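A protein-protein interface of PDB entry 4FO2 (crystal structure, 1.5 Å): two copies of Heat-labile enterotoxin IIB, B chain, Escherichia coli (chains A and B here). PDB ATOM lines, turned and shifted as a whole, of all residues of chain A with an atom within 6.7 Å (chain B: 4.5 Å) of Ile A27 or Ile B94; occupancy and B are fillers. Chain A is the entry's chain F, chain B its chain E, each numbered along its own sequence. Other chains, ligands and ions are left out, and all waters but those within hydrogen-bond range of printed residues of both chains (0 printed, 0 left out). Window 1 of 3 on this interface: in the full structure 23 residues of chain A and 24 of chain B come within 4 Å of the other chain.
No position is printed for both chains.
Hydrophobic or aromatic side chains of chain B within 4 Å of the printed part of chain A: Phe B5, Phe B6, Met B64, Ile B67, Ala B93 and Leu B96. Of the 13 printed residues of chain A, 9 touch a printed residue of chain B. Printed residues of chain A that touch a printed residue of chain B: Lys A25, Tyr A26, Ile A27, Ser A28, Asp A29, Ile A30, Tyr A38, Val A40 and Val A46. Hydrophobic or aromatic side chains of chain A that line the printed part of chain B: Tyr A26, Ile A27, Ile A30, Tyr A38, Val A40 and Val A46. Among the printed residues, 19 pairs touch across the chains.
The backbone carbonyl oxygen (O) of Ser A28 lies within hydrogen-bond range of the backbone NH (N) of Ile B94, at 3.0 Å. The backbone carbonyl oxygen (O) of Tyr A26 lies within hydrogen-bond range of the backbone NH (N) of Leu B96 (2.8 Å).
Of chain B, only Phe B5, Phe B6, Ile B94 and Glu B95 come within 4 Å of Ile A27. Met A37 touches none of the printed residues of chain B. Val A39 touches none of the printed residues of chain B. Of the printed residues of chain A, Ser B3 touches Val A40. Of the printed residues of chain A, Ile B67 touches Tyr A26 (3.6 Å) and Ser A28 (3.96 Å). Of the printed residues of chain A, Glu B95 touches Lys A25 (3.7 Å), Tyr A26 (3.3 Å) and Ile A27 (3.4 Å). Of the printed residues of chain A, Leu B96 touches Lys A25 and Tyr A26. The nearest residue of chain B that does not touch Ile A27 is Ser B3 (4.1 Å). The nearest residue of chain A that does not touch Ile B94 is Asp A29 (5.2 Å). The nearest printed residue of chain B that does not touch Val A46 is Ser B3 (5.9 Å).
Among the printed residues, merely in contact across the chains: Lys A25 with Glu B95, Lys A25 with Leu B96, Tyr A26 with Ile B67, Tyr A26 with Ile B94, Tyr A26 with Glu B95, Ile A27 with Phe B5, Ile A27 with Phe B6, Ile A27 with Ile B94, Ile A27 with Glu B95, Ser A28 with Met B64, Ser A28 with Ile B67, Ser A28 with Ala B93, Asp A29 with Ala B93, Ile A30 with Met B64, Tyr A38 with Phe B5, Val A40 with Ser B3 and Val A46 with Phe B5.
OG of Ser B3 is in hydrogen-bond range of OE2 of Glu B95 (2.5 Å). The backbone carbonyl oxygen (O) of Asp A29 is in hydrogen-bond range of the backbone NH (N) of Gly A36 (2.9 Å). The backbone carbonyl oxygen (O) of Tyr A38 sits at hydrogen-bond distance from the backbone NH (N) of Ile A27 (2.9 Å). The side-chain sulfur of Met A37 lies within hydrogen-bond range of the side-chain hydroxyl of Ser A28 (3.6 Å). The side-chain carboxylate (OE1) of Glu B95 lies close to the side-chain amide oxygen (OD1) of Asn B79 (2.8 Å). The backbone carbonyl oxygen (O) of Lys A25 is in hydrogen-bond range of the backbone NH (N) of Val A40, at 3.1 Å.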
ATOM      1  N   LYS A  25       6.242   6.221 -15.780  1.00  0.00           N
ATOM      2  CA  LYS A  25       6.597   5.606 -17.073  1.00  0.00           C
ATOM      3  C   LYS A  25       8.106   5.361 -17.130  1.00  0.00           C
ATOM      4  O   LYS A  25       8.923   6.182 -16.660  1.00  0.00           O
ATOM      5  CB  LYS A  25       6.280   6.546 -18.282  1.00  0.00           C
ATOM      6  CG  LYS A  25       4.915   7.361 -18.121  1.00  0.00           C
ATOM      7  CD  LYS A  25       3.815   6.648 -18.601  1.00  0.00           C
ATOM      8  CE  LYS A  25       2.612   7.633 -18.855  1.00  0.00           C
ATOM      9  NZ  LYS A  25       1.389   6.897 -18.650  1.00  0.00           N
ATOM     10  N   TYR A  26       8.423   4.343 -17.929  1.00  0.00           N
ATOM     11  CA  TYR A  26       9.843   3.973 -18.131  1.00  0.00           C
ATOM     12  C   TYR A  26       9.986   3.698 -19.629  1.00  0.00           C
ATOM     13  O   TYR A  26       9.262   2.897 -20.211  1.00  0.00           O
ATOM     14  CB  TYR A  26      10.173   2.724 -17.277  1.00  0.00           C
ATOM     15  CG  TYR A  26      11.645   2.260 -17.410  1.00  0.00           C
ATOM     16  CD1 TYR A  26      12.676   3.024 -16.923  1.00  0.00           C
ATOM     17  CD2 TYR A  26      11.952   1.054 -18.022  1.00  0.00           C
ATOM     18  CE1 TYR A  26      14.047   2.571 -16.942  1.00  0.00           C
ATOM     19  CE2 TYR A  26      13.356   0.590 -18.036  1.00  0.00           C
ATOM     20  CZ  TYR A  26      14.329   1.402 -17.575  1.00  0.00           C
ATOM     21  OH  TYR A  26      15.674   0.971 -17.625  1.00  0.00           O
ATOM     22  N   ILE A  27      10.857   4.467 -20.301  1.00  0.00           N
ATOM     23  CA  ILE A  27      10.955   4.490 -21.768  1.00  0.00           C
ATOM     24  C   ILE A  27      12.373   4.027 -22.201  1.00  0.00           C
ATOM     25  O   ILE A  27      13.387   4.491 -21.666  1.00  0.00           O
ATOM     26  CB  ILE A  27      10.821   5.900 -22.253  1.00  0.00           C
ATOM     27  CG1 ILE A  27       9.436   6.500 -21.933  1.00  0.00           C
ATOM     28  CG2 ILE A  27      11.063   5.946 -23.804  1.00  0.00           C
ATOM     29  CD1 ILE A  27       9.340   7.964 -22.107  1.00  0.00           C
ATOM     30  N   SER A  28      12.380   3.097 -23.183  1.00  0.00           N
ATOM     31  CA  SER A  28      13.624   2.795 -23.964  1.00  0.00           C
ATOM     32  C   SER A  28      13.388   3.243 -25.402  1.00  0.00           C
ATOM     33  O   SER A  28      12.379   2.888 -25.943  1.00  0.00           O
ATOM     34  CB  SER A  28      13.731   1.298 -23.981  1.00  0.00           C
ATOM     35  OG  SER A  28      14.927   1.052 -24.737  1.00  0.00           O
ATOM     36  N   ASP A  29      14.318   4.035 -25.971  1.00  0.00           N
ATOM     37  CA  ASP A  29      14.119   4.584 -27.337  1.00  0.00           C
ATOM     38  C   ASP A  29      15.381   4.380 -28.138  1.00  0.00           C
ATOM     39  O   ASP A  29      16.438   4.656 -27.623  1.00  0.00           O
ATOM     40  CB  ASP A  29      13.775   6.037 -27.160  1.00  0.00           C
ATOM     41  CG  ASP A  29      13.411   6.723 -28.480  1.00  0.00           C
ATOM     42  OD1 ASP A  29      14.037   6.453 -29.502  1.00  0.00           O
ATOM     43  OD2 ASP A  29      12.556   7.613 -28.465  1.00  0.00           O
ATOM     44  N   ILE A  30      15.300   3.727 -29.323  1.00  0.00           N
ATOM     45  CA  ILE A  30      16.512   3.660 -30.199  1.00  0.00           C
ATOM     46  C   ILE A  30      16.286   4.432 -31.481  1.00  0.00           C
ATOM     47  O   ILE A  30      17.049   4.246 -32.458  1.00  0.00           O
ATOM     48  CB  ILE A  30      16.989   2.256 -30.578  1.00  0.00           C
ATOM     49  CG1 ILE A  30      15.903   1.434 -31.220  1.00  0.00           C
ATOM     50  CG2 ILE A  30      17.533   1.488 -29.396  1.00  0.00           C
ATOM     51  CD1 ILE A  30      16.574   0.184 -31.886  1.00  0.00           C
ATOM     52  N   GLY A  36      17.766   6.740 -26.125  1.00  0.00           N
ATOM     53  CA  GLY A  36      18.160   6.834 -24.722  1.00  0.00           C
ATOM     54  C   GLY A  36      17.141   6.165 -23.776  1.00  0.00           C
ATOM     55  O   GLY A  36      16.199   5.600 -24.245  1.00  0.00           O
ATOM     56  N   MET A  37      17.403   6.206 -22.468  1.00  0.00           N
ATOM     57  CA  MET A  37      16.481   5.713 -21.476  1.00  0.00           C
ATOM     58  C   MET A  37      15.932   6.903 -20.689  1.00  0.00           C
ATOM     59  O   MET A  37      16.669   7.821 -20.354  1.00  0.00           O
ATOM     60  CB  MET A  37      17.310   4.894 -20.500  1.00  0.00           C
ATOM     61  CG  MET A  37      17.847   3.638 -21.188  1.00  0.00           C
ATOM     62  SD  MET A  37      16.579   2.484 -21.860  1.00  0.00           S
ATOM     63  CE  MET A  37      15.517   2.366 -20.368  1.00  0.00           C
ATOM     64  N   TYR A  38      14.601   6.898 -20.468  1.00  0.00           N
ATOM     65  CA  TYR A  38      13.971   7.998 -19.829  1.00  0.00           C
ATOM     66  C   TYR A  38      12.919   7.565 -18.813  1.00  0.00           C
ATOM     67  O   TYR A  38      12.414   6.466 -18.938  1.00  0.00           O
ATOM     68  CB  TYR A  38      13.187   8.863 -20.876  1.00  0.00           C
ATOM     69  CG  TYR A  38      14.129   9.345 -21.996  1.00  0.00           C
ATOM     70  CD1 TYR A  38      14.245   8.578 -23.132  1.00  0.00           C
ATOM     71  CD2 TYR A  38      14.859  10.541 -21.851  1.00  0.00           C
ATOM     72  CE1 TYR A  38      15.076   9.006 -24.193  1.00  0.00           C
ATOM     73  CE2 TYR A  38      15.676  10.988 -22.917  1.00  0.00           C
ATOM     74  CZ  TYR A  38      15.786  10.181 -24.017  1.00  0.00           C
ATOM     75  OH  TYR A  38      16.560  10.617 -25.122  1.00  0.00           O
ATOM     76  N   VAL A  39      12.604   8.469 -17.887  1.00  0.00           N
ATOM     77  CA  VAL A  39      11.488   8.178 -16.954  1.00  0.00           C
ATOM     78  C   VAL A  39      10.615   9.428 -16.931  1.00  0.00           C
ATOM     79  O   VAL A  39      11.115  10.551 -17.180  1.00  0.00           O
ATOM     80  CB  VAL A  39      11.983   7.882 -15.518  1.00  0.00           C
ATOM     81  CG1 VAL A  39      12.743   6.523 -15.437  1.00  0.00           C
ATOM     82  CG2 VAL A  39      12.911   8.977 -14.940  1.00  0.00           C
ATOM     83  N   VAL A  40       9.310   9.210 -16.632  1.00  0.00           N
ATOM     84  CA  VAL A  40       8.293  10.280 -16.612  1.00  0.00           C
ATOM     85  C   VAL A  40       7.689  10.164 -15.231  1.00  0.00           C
ATOM     86  O   VAL A  40       7.320   9.023 -14.815  1.00  0.00           O
ATOM     87  CB  VAL A  40       7.222  10.113 -17.690  1.00  0.00           C
ATOM     88  CG1 VAL A  40       6.317  11.398 -17.752  1.00  0.00           C
ATOM     89  CG2 VAL A  40       7.917   9.926 -19.086  1.00  0.00           C
ATOM     90  N   VAL A  46      10.072  14.882 -17.033  1.00  0.00           N
ATOM     91  CA  VAL A  46      10.872  13.869 -17.772  1.00  0.00           C
ATOM     92  C   VAL A  46      12.346  13.954 -17.447  1.00  0.00           C
ATOM     93  O   VAL A  46      12.894  15.050 -17.341  1.00  0.00           O
ATOM     94  CB  VAL A  46      10.730  14.072 -19.276  1.00  0.00           C
ATOM     95  CG1 VAL A  46      11.519  13.011 -20.032  1.00  0.00           C
ATOM     96  CG2 VAL A  46       9.290  13.977 -19.638  1.00  0.00           C
ATOM     97  N   ILE A  49      18.039   8.947 -18.124  1.00  0.00           N
ATOM     98  CA  ILE A  49      18.976   8.180 -17.325  1.00  0.00           C
ATOM     99  C   ILE A  49      20.337   8.128 -18.020  1.00  0.00           C
ATOM    100  O   ILE A  49      20.350   7.781 -19.253  1.00  0.00           O
ATOM    101  CB  ILE A  49      18.452   6.741 -17.145  1.00  0.00           C
ATOM    102  CG1 ILE A  49      16.960   6.777 -16.612  1.00  0.00           C
ATOM    103  CG2 ILE A  49      19.471   5.927 -16.229  1.00  0.00           C
ATOM    104  CD1 ILE A  49      16.418   5.406 -16.300  1.00  0.00           C
ATOM    105  N   SER B   3       2.970   9.219 -22.587  1.00  0.00           N
ATOM    106  CA  SER B   3       3.476  10.565 -22.298  1.00  0.00           C
ATOM    107  C   SER B   3       3.503  11.447 -23.546  1.00  0.00           C
ATOM    108  O   SER B   3       3.714  10.937 -24.632  1.00  0.00           O
ATOM    109  CB  SER B   3       4.862  10.554 -21.619  1.00  0.00           C
ATOM    110  OG  SER B   3       5.786   9.879 -22.437  1.00  0.00           O
ATOM    111  N   PHE B   5       5.979  13.292 -24.181  1.00  0.00           N
ATOM    112  CA  PHE B   5       7.391  13.099 -24.553  1.00  0.00           C
ATOM    113  C   PHE B   5       7.476  11.889 -25.468  1.00  0.00           C
ATOM    114  O   PHE B   5       7.972  12.026 -26.582  1.00  0.00           O
ATOM    115  CB  PHE B   5       8.238  12.914 -23.291  1.00  0.00           C
ATOM    116  CG  PHE B   5       9.688  12.684 -23.539  1.00  0.00           C
ATOM    117  CD1 PHE B   5      10.560  13.710 -23.953  1.00  0.00           C
ATOM    118  CD2 PHE B   5      10.235  11.404 -23.322  1.00  0.00           C
ATOM    119  CE1 PHE B   5      11.934  13.462 -24.159  1.00  0.00           C
ATOM    120  CE2 PHE B   5      11.605  11.209 -23.466  1.00  0.00           C
ATOM    121  CZ  PHE B   5      12.419  12.256 -23.906  1.00  0.00           C
ATOM    122  N   PHE B   6       6.934  10.747 -25.057  1.00  0.00           N
ATOM    123  CA  PHE B   6       6.939   9.540 -25.922  1.00  0.00           C
ATOM    124  C   PHE B   6       6.256   9.810 -27.264  1.00  0.00           C
ATOM    125  O   PHE B   6       6.720   9.371 -28.305  1.00  0.00           O
ATOM    126  CB  PHE B   6       6.274   8.367 -25.197  1.00  0.00           C
ATOM    127  CG  PHE B   6       6.438   7.037 -25.927  1.00  0.00           C
ATOM    128  CD1 PHE B   6       7.648   6.362 -25.737  1.00  0.00           C
ATOM    129  CD2 PHE B   6       5.493   6.546 -26.745  1.00  0.00           C
ATOM    130  CE1 PHE B   6       7.898   5.130 -26.350  1.00  0.00           C
ATOM    131  CE2 PHE B   6       5.675   5.347 -27.412  1.00  0.00           C
ATOM    132  CZ  PHE B   6       6.919   4.629 -27.232  1.00  0.00           C
ATOM    133  N   MET B  64      14.426  -2.766 -23.548  1.00  0.00           N
ATOM    134  CA  MET B  64      13.137  -3.057 -24.248  1.00  0.00           C
ATOM    135  C   MET B  64      12.663  -4.465 -23.883  1.00  0.00           C
ATOM    136  O   MET B  64      11.486  -4.638 -23.611  1.00  0.00           O
ATOM    137  CB  MET B  64      13.421  -3.019 -25.774  1.00  0.00           C
ATOM    138  CG  MET B  64      13.459  -1.672 -26.243  1.00  0.00           C
ATOM    139  SD  MET B  64      13.477  -1.793 -28.120  1.00  0.00           S
ATOM    140  CE  MET B  64      13.461  -0.037 -28.497  1.00  0.00           C
ATOM    141  N   ILE B  67      11.310  -4.446 -20.341  1.00  0.00           N
ATOM    142  CA  ILE B  67       9.942  -3.790 -20.317  1.00  0.00           C
ATOM    143  C   ILE B  67       8.965  -4.757 -20.868  1.00  0.00           C
ATOM    144  O   ILE B  67       7.909  -4.942 -20.280  1.00  0.00           O
ATOM    145  CB  ILE B  67       9.949  -2.480 -21.160  1.00  0.00           C
ATOM    146  CG1 ILE B  67      10.772  -1.442 -20.393  1.00  0.00           C
ATOM    147  CG2 ILE B  67       8.460  -2.024 -21.452  1.00  0.00           C
ATOM    148  CD1 ILE B  67      11.185  -0.162 -21.278  1.00  0.00           C
ATOM    149  N   VAL B  78       1.723  -1.178 -22.236  1.00  0.00           N
ATOM    150  CA  VAL B  78       2.855  -0.432 -22.810  1.00  0.00           C
ATOM    151  C   VAL B  78       2.338   0.444 -23.944  1.00  0.00           C
ATOM    152  O   VAL B  78       1.300   0.167 -24.516  1.00  0.00           O
ATOM    153  CB  VAL B  78       3.910  -1.413 -23.371  1.00  0.00           C
ATOM    154  CG1 VAL B  78       4.468  -2.222 -22.144  1.00  0.00           C
ATOM    155  CG2 VAL B  78       3.401  -2.283 -24.466  1.00  0.00           C
ATOM    156  N   ASN B  79       3.102   1.497 -24.282  1.00  0.00           N
ATOM    157  CA  ASN B  79       2.902   2.214 -25.531  1.00  0.00           C
ATOM    158  C   ASN B  79       4.103   1.944 -26.396  1.00  0.00           C
ATOM    159  O   ASN B  79       5.237   1.785 -25.885  1.00  0.00           O
ATOM    160  CB  ASN B  79       2.817   3.721 -25.225  1.00  0.00           C
ATOM    161  CG  ASN B  79       1.817   4.005 -24.055  1.00  0.00           C
ATOM    162  OD1 ASN B  79       2.196   4.538 -22.943  1.00  0.00           O
ATOM    163  ND2 ASN B  79       0.543   3.563 -24.285  1.00  0.00           N
ATOM    164  N   MET B  80       3.895   1.791 -27.712  1.00  0.00           N
ATOM    165  CA  MET B  80       4.998   1.462 -28.618  1.00  0.00           C
ATOM    166  C   MET B  80       5.114   2.468 -29.748  1.00  0.00           C
ATOM    167  O   MET B  80       4.131   3.037 -30.215  1.00  0.00           O
ATOM    168  CB  MET B  80       4.863   0.028 -29.197  1.00  0.00           C
ATOM    169  CG  MET B  80       4.959  -0.993 -28.013  1.00  0.00           C
ATOM    170  SD  MET B  80       4.785  -2.644 -28.643  1.00  0.00           S
ATOM    171  CE  MET B  80       3.321  -2.332 -29.436  1.00  0.00           C
ATOM    172  N   ILE B  91       9.655  -2.824 -32.917  1.00  0.00           N
ATOM    173  CA  ILE B  91       9.573  -1.770 -31.920  1.00  0.00           C
ATOM    174  C   ILE B  91      10.854  -0.981 -31.895  1.00  0.00           C
ATOM    175  O   ILE B  91      11.941  -1.514 -31.613  1.00  0.00           O
ATOM    176  CB  ILE B  91       9.338  -2.398 -30.505  1.00  0.00           C
ATOM    177  CG1 ILE B  91       8.056  -3.199 -30.463  1.00  0.00           C
ATOM    178  CG2 ILE B  91       9.428  -1.319 -29.339  1.00  0.00           C
ATOM    179  CD1 ILE B  91       7.979  -4.222 -29.317  1.00  0.00           C
ATOM    180  N   ALA B  93      10.684   2.130 -30.044  1.00  0.00           N
ATOM    181  CA  ALA B  93      10.644   2.685 -28.669  1.00  0.00           C
ATOM    182  C   ALA B  93       9.496   2.086 -27.970  1.00  0.00           C
ATOM    183  O   ALA B  93       8.502   1.700 -28.594  1.00  0.00           O
ATOM    184  CB  ALA B  93      10.522   4.225 -28.681  1.00  0.00           C
ATOM    185  N   ILE B  94       9.653   1.932 -26.662  1.00  0.00           N
ATOM    186  CA  ILE B  94       8.559   1.339 -25.841  1.00  0.00           C
ATOM    187  C   ILE B  94       8.523   2.098 -24.493  1.00  0.00           C
ATOM    188  O   ILE B  94       9.548   2.525 -23.928  1.00  0.00           O
ATOM    189  CB  ILE B  94       8.761  -0.164 -25.659  1.00  0.00           C
ATOM    190  CG1 ILE B  94       7.507  -0.791 -25.032  1.00  0.00           C
ATOM    191  CG2 ILE B  94      10.078  -0.514 -24.803  1.00  0.00           C
ATOM    192  CD1 ILE B  94       7.510  -2.338 -25.229  1.00  0.00           C
ATOM    193  N   GLU B  95       7.305   2.288 -23.970  1.00  0.00           N
ATOM    194  CA  GLU B  95       7.098   2.976 -22.744  1.00  0.00           C
ATOM    195  C   GLU B  95       6.230   2.059 -21.843  1.00  0.00           C
ATOM    196  O   GLU B  95       5.090   1.724 -22.208  1.00  0.00           O
ATOM    197  CB  GLU B  95       6.274   4.251 -23.039  1.00  0.00           C
ATOM    198  CG  GLU B  95       5.903   5.036 -21.732  1.00  0.00           C
ATOM    199  CD  GLU B  95       5.353   6.429 -22.065  1.00  0.00           C
ATOM    200  OE1 GLU B  95       4.268   6.449 -22.642  1.00  0.00           O
ATOM    201  OE2 GLU B  95       5.966   7.444 -21.819  1.00  0.00           O
ATOM    202  N   LEU B  96       6.779   1.659 -20.686  1.00  0.00           N
ATOM    203  CA  LEU B  96       6.045   0.818 -19.714  1.00  0.00           C
ATOM    204  C   LEU B  96       5.278   1.771 -18.815  1.00  0.00           C
ATOM    205  O   LEU B  96       5.794   2.773 -18.346  1.00  0.00           O
ATOM    206  CB  LEU B  96       7.108   0.169 -18.847  1.00  0.00           C
ATOM    207  CG  LEU B  96       6.479  -0.681 -17.723  1.00  0.00           C
ATOM    208  CD1 LEU B  96       5.690  -1.816 -18.351  1.00  0.00           C
ATOM    209  CD2 LEU B  96       7.643  -1.256 -16.900  1.00  0.00           C
